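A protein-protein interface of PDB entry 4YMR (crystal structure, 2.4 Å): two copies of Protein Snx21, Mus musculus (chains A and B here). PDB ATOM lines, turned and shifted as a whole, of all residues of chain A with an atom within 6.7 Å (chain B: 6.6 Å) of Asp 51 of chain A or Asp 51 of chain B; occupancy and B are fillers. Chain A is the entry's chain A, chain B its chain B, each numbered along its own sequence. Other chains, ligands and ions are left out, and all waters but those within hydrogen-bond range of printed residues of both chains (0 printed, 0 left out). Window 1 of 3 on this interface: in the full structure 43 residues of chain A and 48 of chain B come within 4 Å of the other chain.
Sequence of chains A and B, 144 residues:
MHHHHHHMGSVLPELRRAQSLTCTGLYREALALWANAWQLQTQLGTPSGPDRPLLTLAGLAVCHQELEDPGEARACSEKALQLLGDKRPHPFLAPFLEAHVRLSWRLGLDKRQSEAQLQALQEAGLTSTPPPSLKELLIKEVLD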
ATOM      1  N   GLN A  41      25.887  16.437 -30.780  1.00  0.00           N
ATOM      2  CA  GLN A  41      24.799  17.371 -31.043  1.00  0.00           C
ATOM      3  C   GLN A  41      24.363  17.417 -32.506  1.00  0.00           C
ATOM      4  O   GLN A  41      23.173  17.540 -32.791  1.00  0.00           O
ATOM      5  CB  GLN A  41      25.192  18.786 -30.592  1.00  0.00           C
ATOM      6  CG  GLN A  41      25.550  18.903 -29.117  1.00  0.00           C
ATOM      7  CD  GLN A  41      26.021  20.307 -28.748  1.00  0.00           C
ATOM      8  OE1 GLN A  41      25.231  21.251 -28.710  1.00  0.00           O
ATOM      9  NE2 GLN A  41      27.315  20.446 -28.485  1.00  0.00           N
ATOM     10  N   GLY A  49      18.027  23.241 -28.848  1.00  0.00           N
ATOM     11  CA  GLY A  49      18.104  24.687 -28.638  1.00  0.00           C
ATOM     12  C   GLY A  49      19.516  25.262 -28.607  1.00  0.00           C
ATOM     13  O   GLY A  49      20.317  24.879 -27.748  1.00  0.00           O
ATOM     14  N   PRO A  50      19.789  26.239 -29.499  1.00  0.00           N
ATOM     15  CA  PRO A  50      21.065  26.737 -30.060  1.00  0.00           C
ATOM     16  C   PRO A  50      21.955  27.696 -29.227  1.00  0.00           C
ATOM     17  O   PRO A  50      22.594  28.551 -29.821  1.00  0.00           O
ATOM     18  CB  PRO A  50      20.610  27.463 -31.327  1.00  0.00           C
ATOM     19  CG  PRO A  50      19.261  27.993 -30.969  1.00  0.00           C
ATOM     20  CD  PRO A  50      18.640  27.031 -29.977  1.00  0.00           C
ATOM     21  N   ASP A  51      22.013  27.556 -27.911  1.00  0.00           N
ATOM     22  CA  ASP A  51      23.028  28.239 -27.124  1.00  0.00           C
ATOM     23  C   ASP A  51      24.139  27.240 -26.802  1.00  0.00           C
ATOM     24  O   ASP A  51      25.297  27.616 -26.615  1.00  0.00           O
ATOM     25  CB  ASP A  51      22.433  28.796 -25.822  1.00  0.00           C
ATOM     26  CG  ASP A  51      21.278  29.756 -26.062  1.00  0.00           C
ATOM     27  OD1 ASP A  51      20.984  30.046 -27.236  1.00  0.00           O
ATOM     28  OD2 ASP A  51      20.673  30.220 -25.068  1.00  0.00           O
ATOM     29  N   ARG A  52      23.753  25.968 -26.724  1.00  0.00           N
ATOM     30  CA  ARG A  52      24.687  24.873 -26.512  1.00  0.00           C
ATOM     31  C   ARG A  52      25.567  24.589 -27.740  1.00  0.00           C
ATOM     32  O   ARG A  52      26.777  24.356 -27.590  1.00  0.00           O
ATOM     33  CB  ARG A  52      23.959  23.602 -26.058  1.00  0.00           C
ATOM     34  CG  ARG A  52      24.175  23.283 -24.603  1.00  0.00           C
ATOM     35  CD  ARG A  52      23.647  21.904 -24.247  1.00  0.00           C
ATOM     36  NE  ARG A  52      22.199  21.892 -24.045  1.00  0.00           N
ATOM     37  CZ  ARG A  52      21.600  22.194 -22.896  1.00  0.00           C
ATOM     38  NH1 ARG A  52      22.323  22.541 -21.840  1.00  0.00           N
ATOM     39  NH2 ARG A  52      20.276  22.156 -22.802  1.00  0.00           N
ATOM     40  N   PRO A  53      24.968  24.582 -28.955  1.00  0.00           N
ATOM     41  CA  PRO A  53      25.831  24.491 -30.137  1.00  0.00           C
ATOM     42  C   PRO A  53      26.798  25.667 -30.222  1.00  0.00           C
ATOM     43  O   PRO A  53      27.985  25.465 -30.418  1.00  0.00           O
ATOM     44  CB  PRO A  53      24.832  24.513 -31.296  1.00  0.00           C
ATOM     45  CG  PRO A  53      23.628  23.911 -30.724  1.00  0.00           C
ATOM     46  CD  PRO A  53      23.551  24.434 -29.328  1.00  0.00           C
ATOM     47  N   LEU A  54      26.285  26.874 -30.035  1.00  0.00           N
ATOM     48  CA  LEU A  54      27.100  28.071 -30.044  1.00  0.00           C
ATOM     49  C   LEU A  54      28.211  28.049 -28.996  1.00  0.00           C
ATOM     50  O   LEU A  54      29.333  28.473 -29.276  1.00  0.00           O
ATOM     51  CB  LEU A  54      26.212  29.314 -29.902  1.00  0.00           C
ATOM     52  CG  LEU A  54      25.366  29.582 -31.151  1.00  0.00           C
ATOM     53  CD1 LEU A  54      24.437  30.761 -30.909  1.00  0.00           C
ATOM     54  CD2 LEU A  54      26.268  29.866 -32.341  1.00  0.00           C
ATOM     55  N   LEU A  55      27.901  27.553 -27.798  1.00  0.00           N
ATOM     56  CA  LEU A  55      28.912  27.415 -26.752  1.00  0.00           C
ATOM     57  C   LEU A  55      30.005  26.425 -27.175  1.00  0.00           C
ATOM     58  O   LEU A  55      31.196  26.643 -26.939  1.00  0.00           O
ATOM     59  CB  LEU A  55      28.292  26.959 -25.432  1.00  0.00           C
ATOM     60  CG  LEU A  55      29.305  26.960 -24.285  1.00  0.00           C
ATOM     61  CD1 LEU A  55      29.299  28.318 -23.607  1.00  0.00           C
ATOM     62  CD2 LEU A  55      29.018  25.869 -23.291  1.00  0.00           C
ATOM     63  N   THR A  56      29.579  25.330 -27.794  1.00  0.00           N
ATOM     64  CA  THR A  56      30.488  24.340 -28.323  1.00  0.00           C
ATOM     65  C   THR A  56      31.426  24.921 -29.379  1.00  0.00           C
ATOM     66  O   THR A  56      32.635  24.720 -29.323  1.00  0.00           O
ATOM     67  CB  THR A  56      29.711  23.182 -28.942  1.00  0.00           C
ATOM     68  OG1 THR A  56      28.748  22.706 -27.999  1.00  0.00           O
ATOM     69  CG2 THR A  56      30.654  22.072 -29.341  1.00  0.00           C
ATOM     70  N   HIS A  90      13.713  28.732 -31.685  1.00  0.00           N
ATOM     71  CA  HIS A  90      13.845  28.223 -30.304  1.00  0.00           C
ATOM     72  C   HIS A  90      12.702  27.235 -30.044  1.00  0.00           C
ATOM     73  O   HIS A  90      11.522  27.571 -30.216  1.00  0.00           O
ATOM     74  CB  HIS A  90      13.892  29.321 -29.222  1.00  0.00           C
ATOM     75  CG  HIS A  90      14.314  28.834 -27.862  1.00  0.00           C
ATOM     76  ND1 HIS A  90      13.693  27.791 -27.206  1.00  0.00           N
ATOM     77  CD2 HIS A  90      15.283  29.280 -27.026  1.00  0.00           C
ATOM     78  CE1 HIS A  90      14.279  27.597 -26.037  1.00  0.00           C
ATOM     79  NE2 HIS A  90      15.237  28.490 -25.898  1.00  0.00           N
ATOM     80  N   PRO A  91      13.061  26.004 -29.636  1.00  0.00           N
ATOM     81  CA  PRO A  91      12.118  24.891 -29.524  1.00  0.00           C
ATOM     82  C   PRO A  91      10.905  25.240 -28.682  1.00  0.00           C
ATOM     83  O   PRO A  91       9.828  24.810 -29.045  1.00  0.00           O
ATOM     84  CB  PRO A  91      12.947  23.775 -28.863  1.00  0.00           C
ATOM     85  CG  PRO A  91      14.162  24.458 -28.304  1.00  0.00           C
ATOM     86  CD  PRO A  91      14.420  25.607 -29.222  1.00  0.00           C
ATOM     87  N   PHE A  92      11.077  26.025 -27.621  1.00  0.00           N
ATOM     88  CA  PHE A  92       9.972  26.381 -26.731  1.00  0.00           C
ATOM     89  C   PHE A  92       8.980  27.432 -27.261  1.00  0.00           C
ATOM     90  O   PHE A  92       7.986  27.708 -26.601  1.00  0.00           O
ATOM     91  CB  PHE A  92      10.508  26.818 -25.371  1.00  0.00           C
ATOM     92  CG  PHE A  92      10.594  25.702 -24.379  1.00  0.00           C
ATOM     93  CD1 PHE A  92       9.480  24.919 -24.106  1.00  0.00           C
ATOM     94  CD2 PHE A  92      11.790  25.415 -23.735  1.00  0.00           C
ATOM     95  CE1 PHE A  92       9.547  23.880 -23.195  1.00  0.00           C
ATOM     96  CE2 PHE A  92      11.874  24.377 -22.822  1.00  0.00           C
ATOM     97  CZ  PHE A  92      10.749  23.607 -22.550  1.00  0.00           C
ATOM     98  N   GLN B  41      16.383  31.054  -9.011  1.00  0.00           N
ATOM     99  CA  GLN B  41      16.999  31.568 -10.222  1.00  0.00           C
ATOM    100  C   GLN B  41      16.848  33.073 -10.267  1.00  0.00           C
ATOM    101  O   GLN B  41      17.511  33.762 -11.052  1.00  0.00           O
ATOM    102  CB  GLN B  41      16.339  30.957 -11.444  1.00  0.00           C
ATOM    103  CG  GLN B  41      16.573  29.477 -11.577  1.00  0.00           C
ATOM    104  CD  GLN B  41      15.837  28.903 -12.756  1.00  0.00           C
ATOM    105  OE1 GLN B  41      16.114  29.253 -13.902  1.00  0.00           O
ATOM    106  NE2 GLN B  41      14.873  28.034 -12.483  1.00  0.00           N
ATOM    107  N   GLY B  49      20.891  33.681 -20.385  1.00  0.00           N
ATOM    108  CA  GLY B  49      20.650  32.568 -21.290  1.00  0.00           C
ATOM    109  C   GLY B  49      19.337  31.857 -21.004  1.00  0.00           C
ATOM    110  O   GLY B  49      19.275  31.011 -20.108  1.00  0.00           O
ATOM    111  N   PRO B  50      18.287  32.175 -21.791  1.00  0.00           N
ATOM    112  CA  PRO B  50      16.906  31.740 -21.536  1.00  0.00           C
ATOM    113  C   PRO B  50      16.680  30.274 -21.895  1.00  0.00           C
ATOM    114  O   PRO B  50      16.375  29.947 -23.042  1.00  0.00           O
ATOM    115  CB  PRO B  50      16.084  32.650 -22.456  1.00  0.00           C
ATOM    116  CG  PRO B  50      16.987  32.882 -23.627  1.00  0.00           C
ATOM    117  CD  PRO B  50      18.404  32.890 -23.078  1.00  0.00           C
ATOM    118  N   ASP B  51      16.849  29.399 -20.912  1.00  0.00           N
ATOM    119  CA  ASP B  51      16.617  27.975 -21.108  1.00  0.00           C
ATOM    120  C   ASP B  51      16.159  27.340 -19.810  1.00  0.00           C
ATOM    121  O   ASP B  51      15.106  26.712 -19.767  1.00  0.00           O
ATOM    122  CB  ASP B  51      17.855  27.276 -21.666  1.00  0.00           C
ATOM    123  CG  ASP B  51      17.845  27.206 -23.180  1.00  0.00           C
ATOM    124  OD1 ASP B  51      16.741  27.288 -23.756  1.00  0.00           O
ATOM    125  OD2 ASP B  51      18.931  27.067 -23.792  1.00  0.00           O
ATOM    126  N   ARG B  52      16.945  27.503 -18.751  1.00  0.00           N
ATOM    127  CA  ARG B  52      16.438  27.172 -17.420  1.00  0.00           C
ATOM    128  C   ARG B  52      15.153  27.952 -17.073  1.00  0.00           C
ATOM    129  O   ARG B  52      14.183  27.334 -16.626  1.00  0.00           O
ATOM    130  CB  ARG B  52      17.516  27.277 -16.326  1.00  0.00           C
ATOM    131  CG  ARG B  52      18.279  25.980 -16.138  1.00  0.00           C
ATOM    132  CD  ARG B  52      19.313  26.060 -15.039  1.00  0.00           C
ATOM    133  NE  ARG B  52      20.359  25.051 -15.217  1.00  0.00           N
ATOM    134  CZ  ARG B  52      21.422  25.208 -16.002  1.00  0.00           C
ATOM    135  NH1 ARG B  52      21.584  26.337 -16.680  1.00  0.00           N
ATOM    136  NH2 ARG B  52      22.323  24.239 -16.107  1.00  0.00           N
ATOM    137  N   PRO B  53      15.136  29.296 -17.285  1.00  0.00           N
ATOM    138  CA  PRO B  53      13.878  30.043 -17.119  1.00  0.00           C
ATOM    139  C   PRO B  53      12.731  29.501 -17.973  1.00  0.00           C
ATOM    140  O   PRO B  53      11.670  29.204 -17.433  1.00  0.00           O
ATOM    141  CB  PRO B  53      14.257  31.467 -17.557  1.00  0.00           C
ATOM    142  CG  PRO B  53      15.705  31.579 -17.191  1.00  0.00           C
ATOM    143  CD  PRO B  53      16.277  30.213 -17.505  1.00  0.00           C
ATOM    144  N   LEU B  54      12.941  29.382 -19.279  1.00  0.00           N
ATOM    145  CA  LEU B  54      11.922  28.828 -20.166  1.00  0.00           C
ATOM    146  C   LEU B  54      11.393  27.473 -19.701  1.00  0.00           C
ATOM    147  O   LEU B  54      10.194  27.218 -19.781  1.00  0.00           O
ATOM    148  CB  LEU B  54      12.438  28.742 -21.598  1.00  0.00           C
ATOM    149  CG  LEU B  54      12.335  30.115 -22.260  1.00  0.00           C
ATOM    150  CD1 LEU B  54      12.786  30.035 -23.701  1.00  0.00           C
ATOM    151  CD2 LEU B  54      10.898  30.629 -22.164  1.00  0.00           C
ATOM    152  N   LEU B  55      12.288  26.631 -19.187  1.00  0.00           N
ATOM    153  CA  LEU B  55      11.935  25.286 -18.736  1.00  0.00           C
ATOM    154  C   LEU B  55      11.211  25.292 -17.400  1.00  0.00           C
ATOM    155  O   LEU B  55      10.305  24.481 -17.179  1.00  0.00           O
ATOM    156  CB  LEU B  55      13.161  24.369 -18.668  1.00  0.00           C
ATOM    157  CG  LEU B  55      12.810  22.891 -18.428  1.00  0.00           C
ATOM    158  CD1 LEU B  55      13.241  22.064 -19.611  1.00  0.00           C
ATOM    159  CD2 LEU B  55      13.378  22.329 -17.120  1.00  0.00           C
ATOM    160  N   THR B  56      11.594  26.197 -16.504  1.00  0.00           N
ATOM    161  CA  THR B  56      10.844  26.329 -15.260  1.00  0.00           C
ATOM    162  C   THR B  56       9.433  26.827 -15.571  1.00  0.00           C
ATOM    163  O   THR B  56       8.453  26.345 -14.996  1.00  0.00           O
ATOM    164  CB  THR B  56      11.537  27.262 -14.241  1.00  0.00           C
ATOM    165  OG1 THR B  56      12.883  26.830 -14.031  1.00  0.00           O
ATOM    166  CG2 THR B  56      10.801  27.237 -12.901  1.00  0.00           C
ATOM    167  N   HIS B  90      21.795  38.149 -29.962  1.00  0.00           N
ATOM    168  CA  HIS B  90      22.343  37.021 -29.254  1.00  0.00           C
ATOM    169  C   HIS B  90      23.725  37.402 -28.713  1.00  0.00           C
ATOM    170  O   HIS B  90      24.533  37.984 -29.436  1.00  0.00           O
ATOM    171  CB  HIS B  90      22.450  35.815 -30.166  1.00  0.00           C
ATOM    172  CG  HIS B  90      22.695  34.555 -29.417  1.00  0.00           C
ATOM    173  ND1 HIS B  90      23.851  34.342 -28.699  1.00  0.00           N
ATOM    174  CD2 HIS B  90      21.912  33.478 -29.210  1.00  0.00           C
ATOM    175  CE1 HIS B  90      23.775  33.170 -28.099  1.00  0.00           C
ATOM    176  NE2 HIS B  90      22.611  32.627 -28.390  1.00  0.00           N
ATOM    177  N   PHE B  92      26.347  35.882 -28.316  1.00  0.00           N
ATOM    178  CA  PHE B  92      27.475  35.298 -29.018  1.00  0.00           C
ATOM    179  C   PHE B  92      27.725  35.921 -30.378  1.00  0.00           C
ATOM    180  O   PHE B  92      28.762  35.667 -30.987  1.00  0.00           O
ATOM    181  CB  PHE B  92      27.304  33.791 -29.167  1.00  0.00           C
ATOM    182  CG  PHE B  92      27.900  33.014 -28.042  1.00  0.00           C
ATOM    183  CD1 PHE B  92      29.276  32.941 -27.892  1.00  0.00           C
ATOM    184  CD2 PHE B  92      27.094  32.357 -27.130  1.00  0.00           C
ATOM    185  CE1 PHE B  92      29.836  32.229 -26.849  1.00  0.00           C
ATOM    186  CE2 PHE B  92      27.650  31.635 -26.091  1.00  0.00           C
ATOM    187  CZ  PHE B  92      29.023  31.573 -25.949  1.00  0.00           C
ATOM    188  N   GLU B 141      29.946  31.767 -18.738  1.00  0.00           N
ATOM    189  CA  GLU B 141      28.798  30.874 -18.837  1.00  0.00           C
ATOM    190  C   GLU B 141      28.757  29.804 -17.752  1.00  0.00           C
ATOM    191  O   GLU B 141      29.776  29.223 -17.390  1.00  0.00           O
ATOM    192  CB  GLU B 141      28.713  30.262 -20.227  1.00  0.00           C
ATOM    193  CG  GLU B 141      27.922  31.122 -21.193  1.00  0.00           C
ATOM    194  CD  GLU B 141      26.478  30.667 -21.310  1.00  0.00           C
ATOM    195  OE1 GLU B 141      26.232  29.444 -21.186  1.00  0.00           O
ATOM    196  OE2 GLU B 141      25.595  31.529 -21.530  1.00  0.00           O
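ND1 of His 90 of chain A lies close to N of Phe 92 of chain A, at 3.2 Å. A ring nitrogen (ND1) of His 90 of chain B lies within hydrogen-bond range of the backbone NH of Phe 92 of chain B (3.0 Å).
NE2 of His 90 of chain A sits at hydrogen-bond distance from O of Pro 50 of chain B (3.4 Å). The side-chain carboxylate (OD1) of Asp 51 of chain A sits at hydrogen-bond distance from a ring nitrogen (NE2) of His 90 of chain B, at 3.3 Å. A ring nitrogen (NE2) of His 90 of chain A is in hydrogen-bond range of the side-chain carboxylate (OD1) of Asp 51 of chain B (2.9 Å).
Hydrophobic or aromatic side chains of chain A within 4 Å of the printed part of chain B: Leu 54, Leu 55 and His 90. Of the 12 printed residues of chain B, 5 touch a printed residue of chain A. Hydrophobic or aromatic side chains of chain B within 4 Å of the printed part of chain A: Leu 54 and His 90. Among the printed residues, 7 pairs touch across the chains.
Asp 51 of chain A touches its own counterpart, Asp 51 of chain B. Asp 51 of chain A touches His 90 of chain B, and with the chains exchanged His 90 of chain A touches Asp 51 of chain B. Leu 54 of chain A touches His 90 of chain B, and with the chains exchanged His 90 of chain A touches Leu 54 of chain B. His 90 of chain A touches Pro 50 of chain B, but with the chains exchanged Pro 50 of chain A does not touch His 90 of chain B (4.3 Å). 11 positions are printed for both chains. Of the 7 pairs that touch across the chains among the printed residues, 5 have their exchanged pair printed and touching as well.
Of chain B, only Asp 51 and His 90 come within 4 Å of Asp 51 of chain A. Printed residues of chain B within 4 Å of Leu 55 of chain A: Glu 141. Pro 91 of chain A touches none of the printed residues of chain B. Of the printed residues of chain A, Pro 50 of chain B touches His 90 (3.4 Å). Of chain A, only Asp 51 (3.8 Å) and His 90 (2.9 Å) come within 4 Å of Asp 51 of chain B. Printed residues of chain A within 4 Å of Leu 54 of chain B: His 90 (3.6 Å). Of the printed residues of chain A, His 90 of chain B touches Asp 51 and Leu 54. Printed residues of chain A within 4 Å of Glu 141 of chain B: Leu 55. The nearest residue of chain B that does not touch Asp 51 of chain A is Pro 50 of chain B (4.03 Å). The nearest residue of chain A that does not touch Asp 51 of chain B is Gly 49 of chain A (4.7 Å).
Asp 51 of chain B touches Asp 51 of chain A. Leu 54 of chain A touches His 90 of chain B. Leu 55 of chain A touches Glu 141 of chain B (CD1 to CB, 3.9 Å). NE2 of His 90 of chain A touches CD1 of Leu 54 of chain B, 3.6 Å away.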
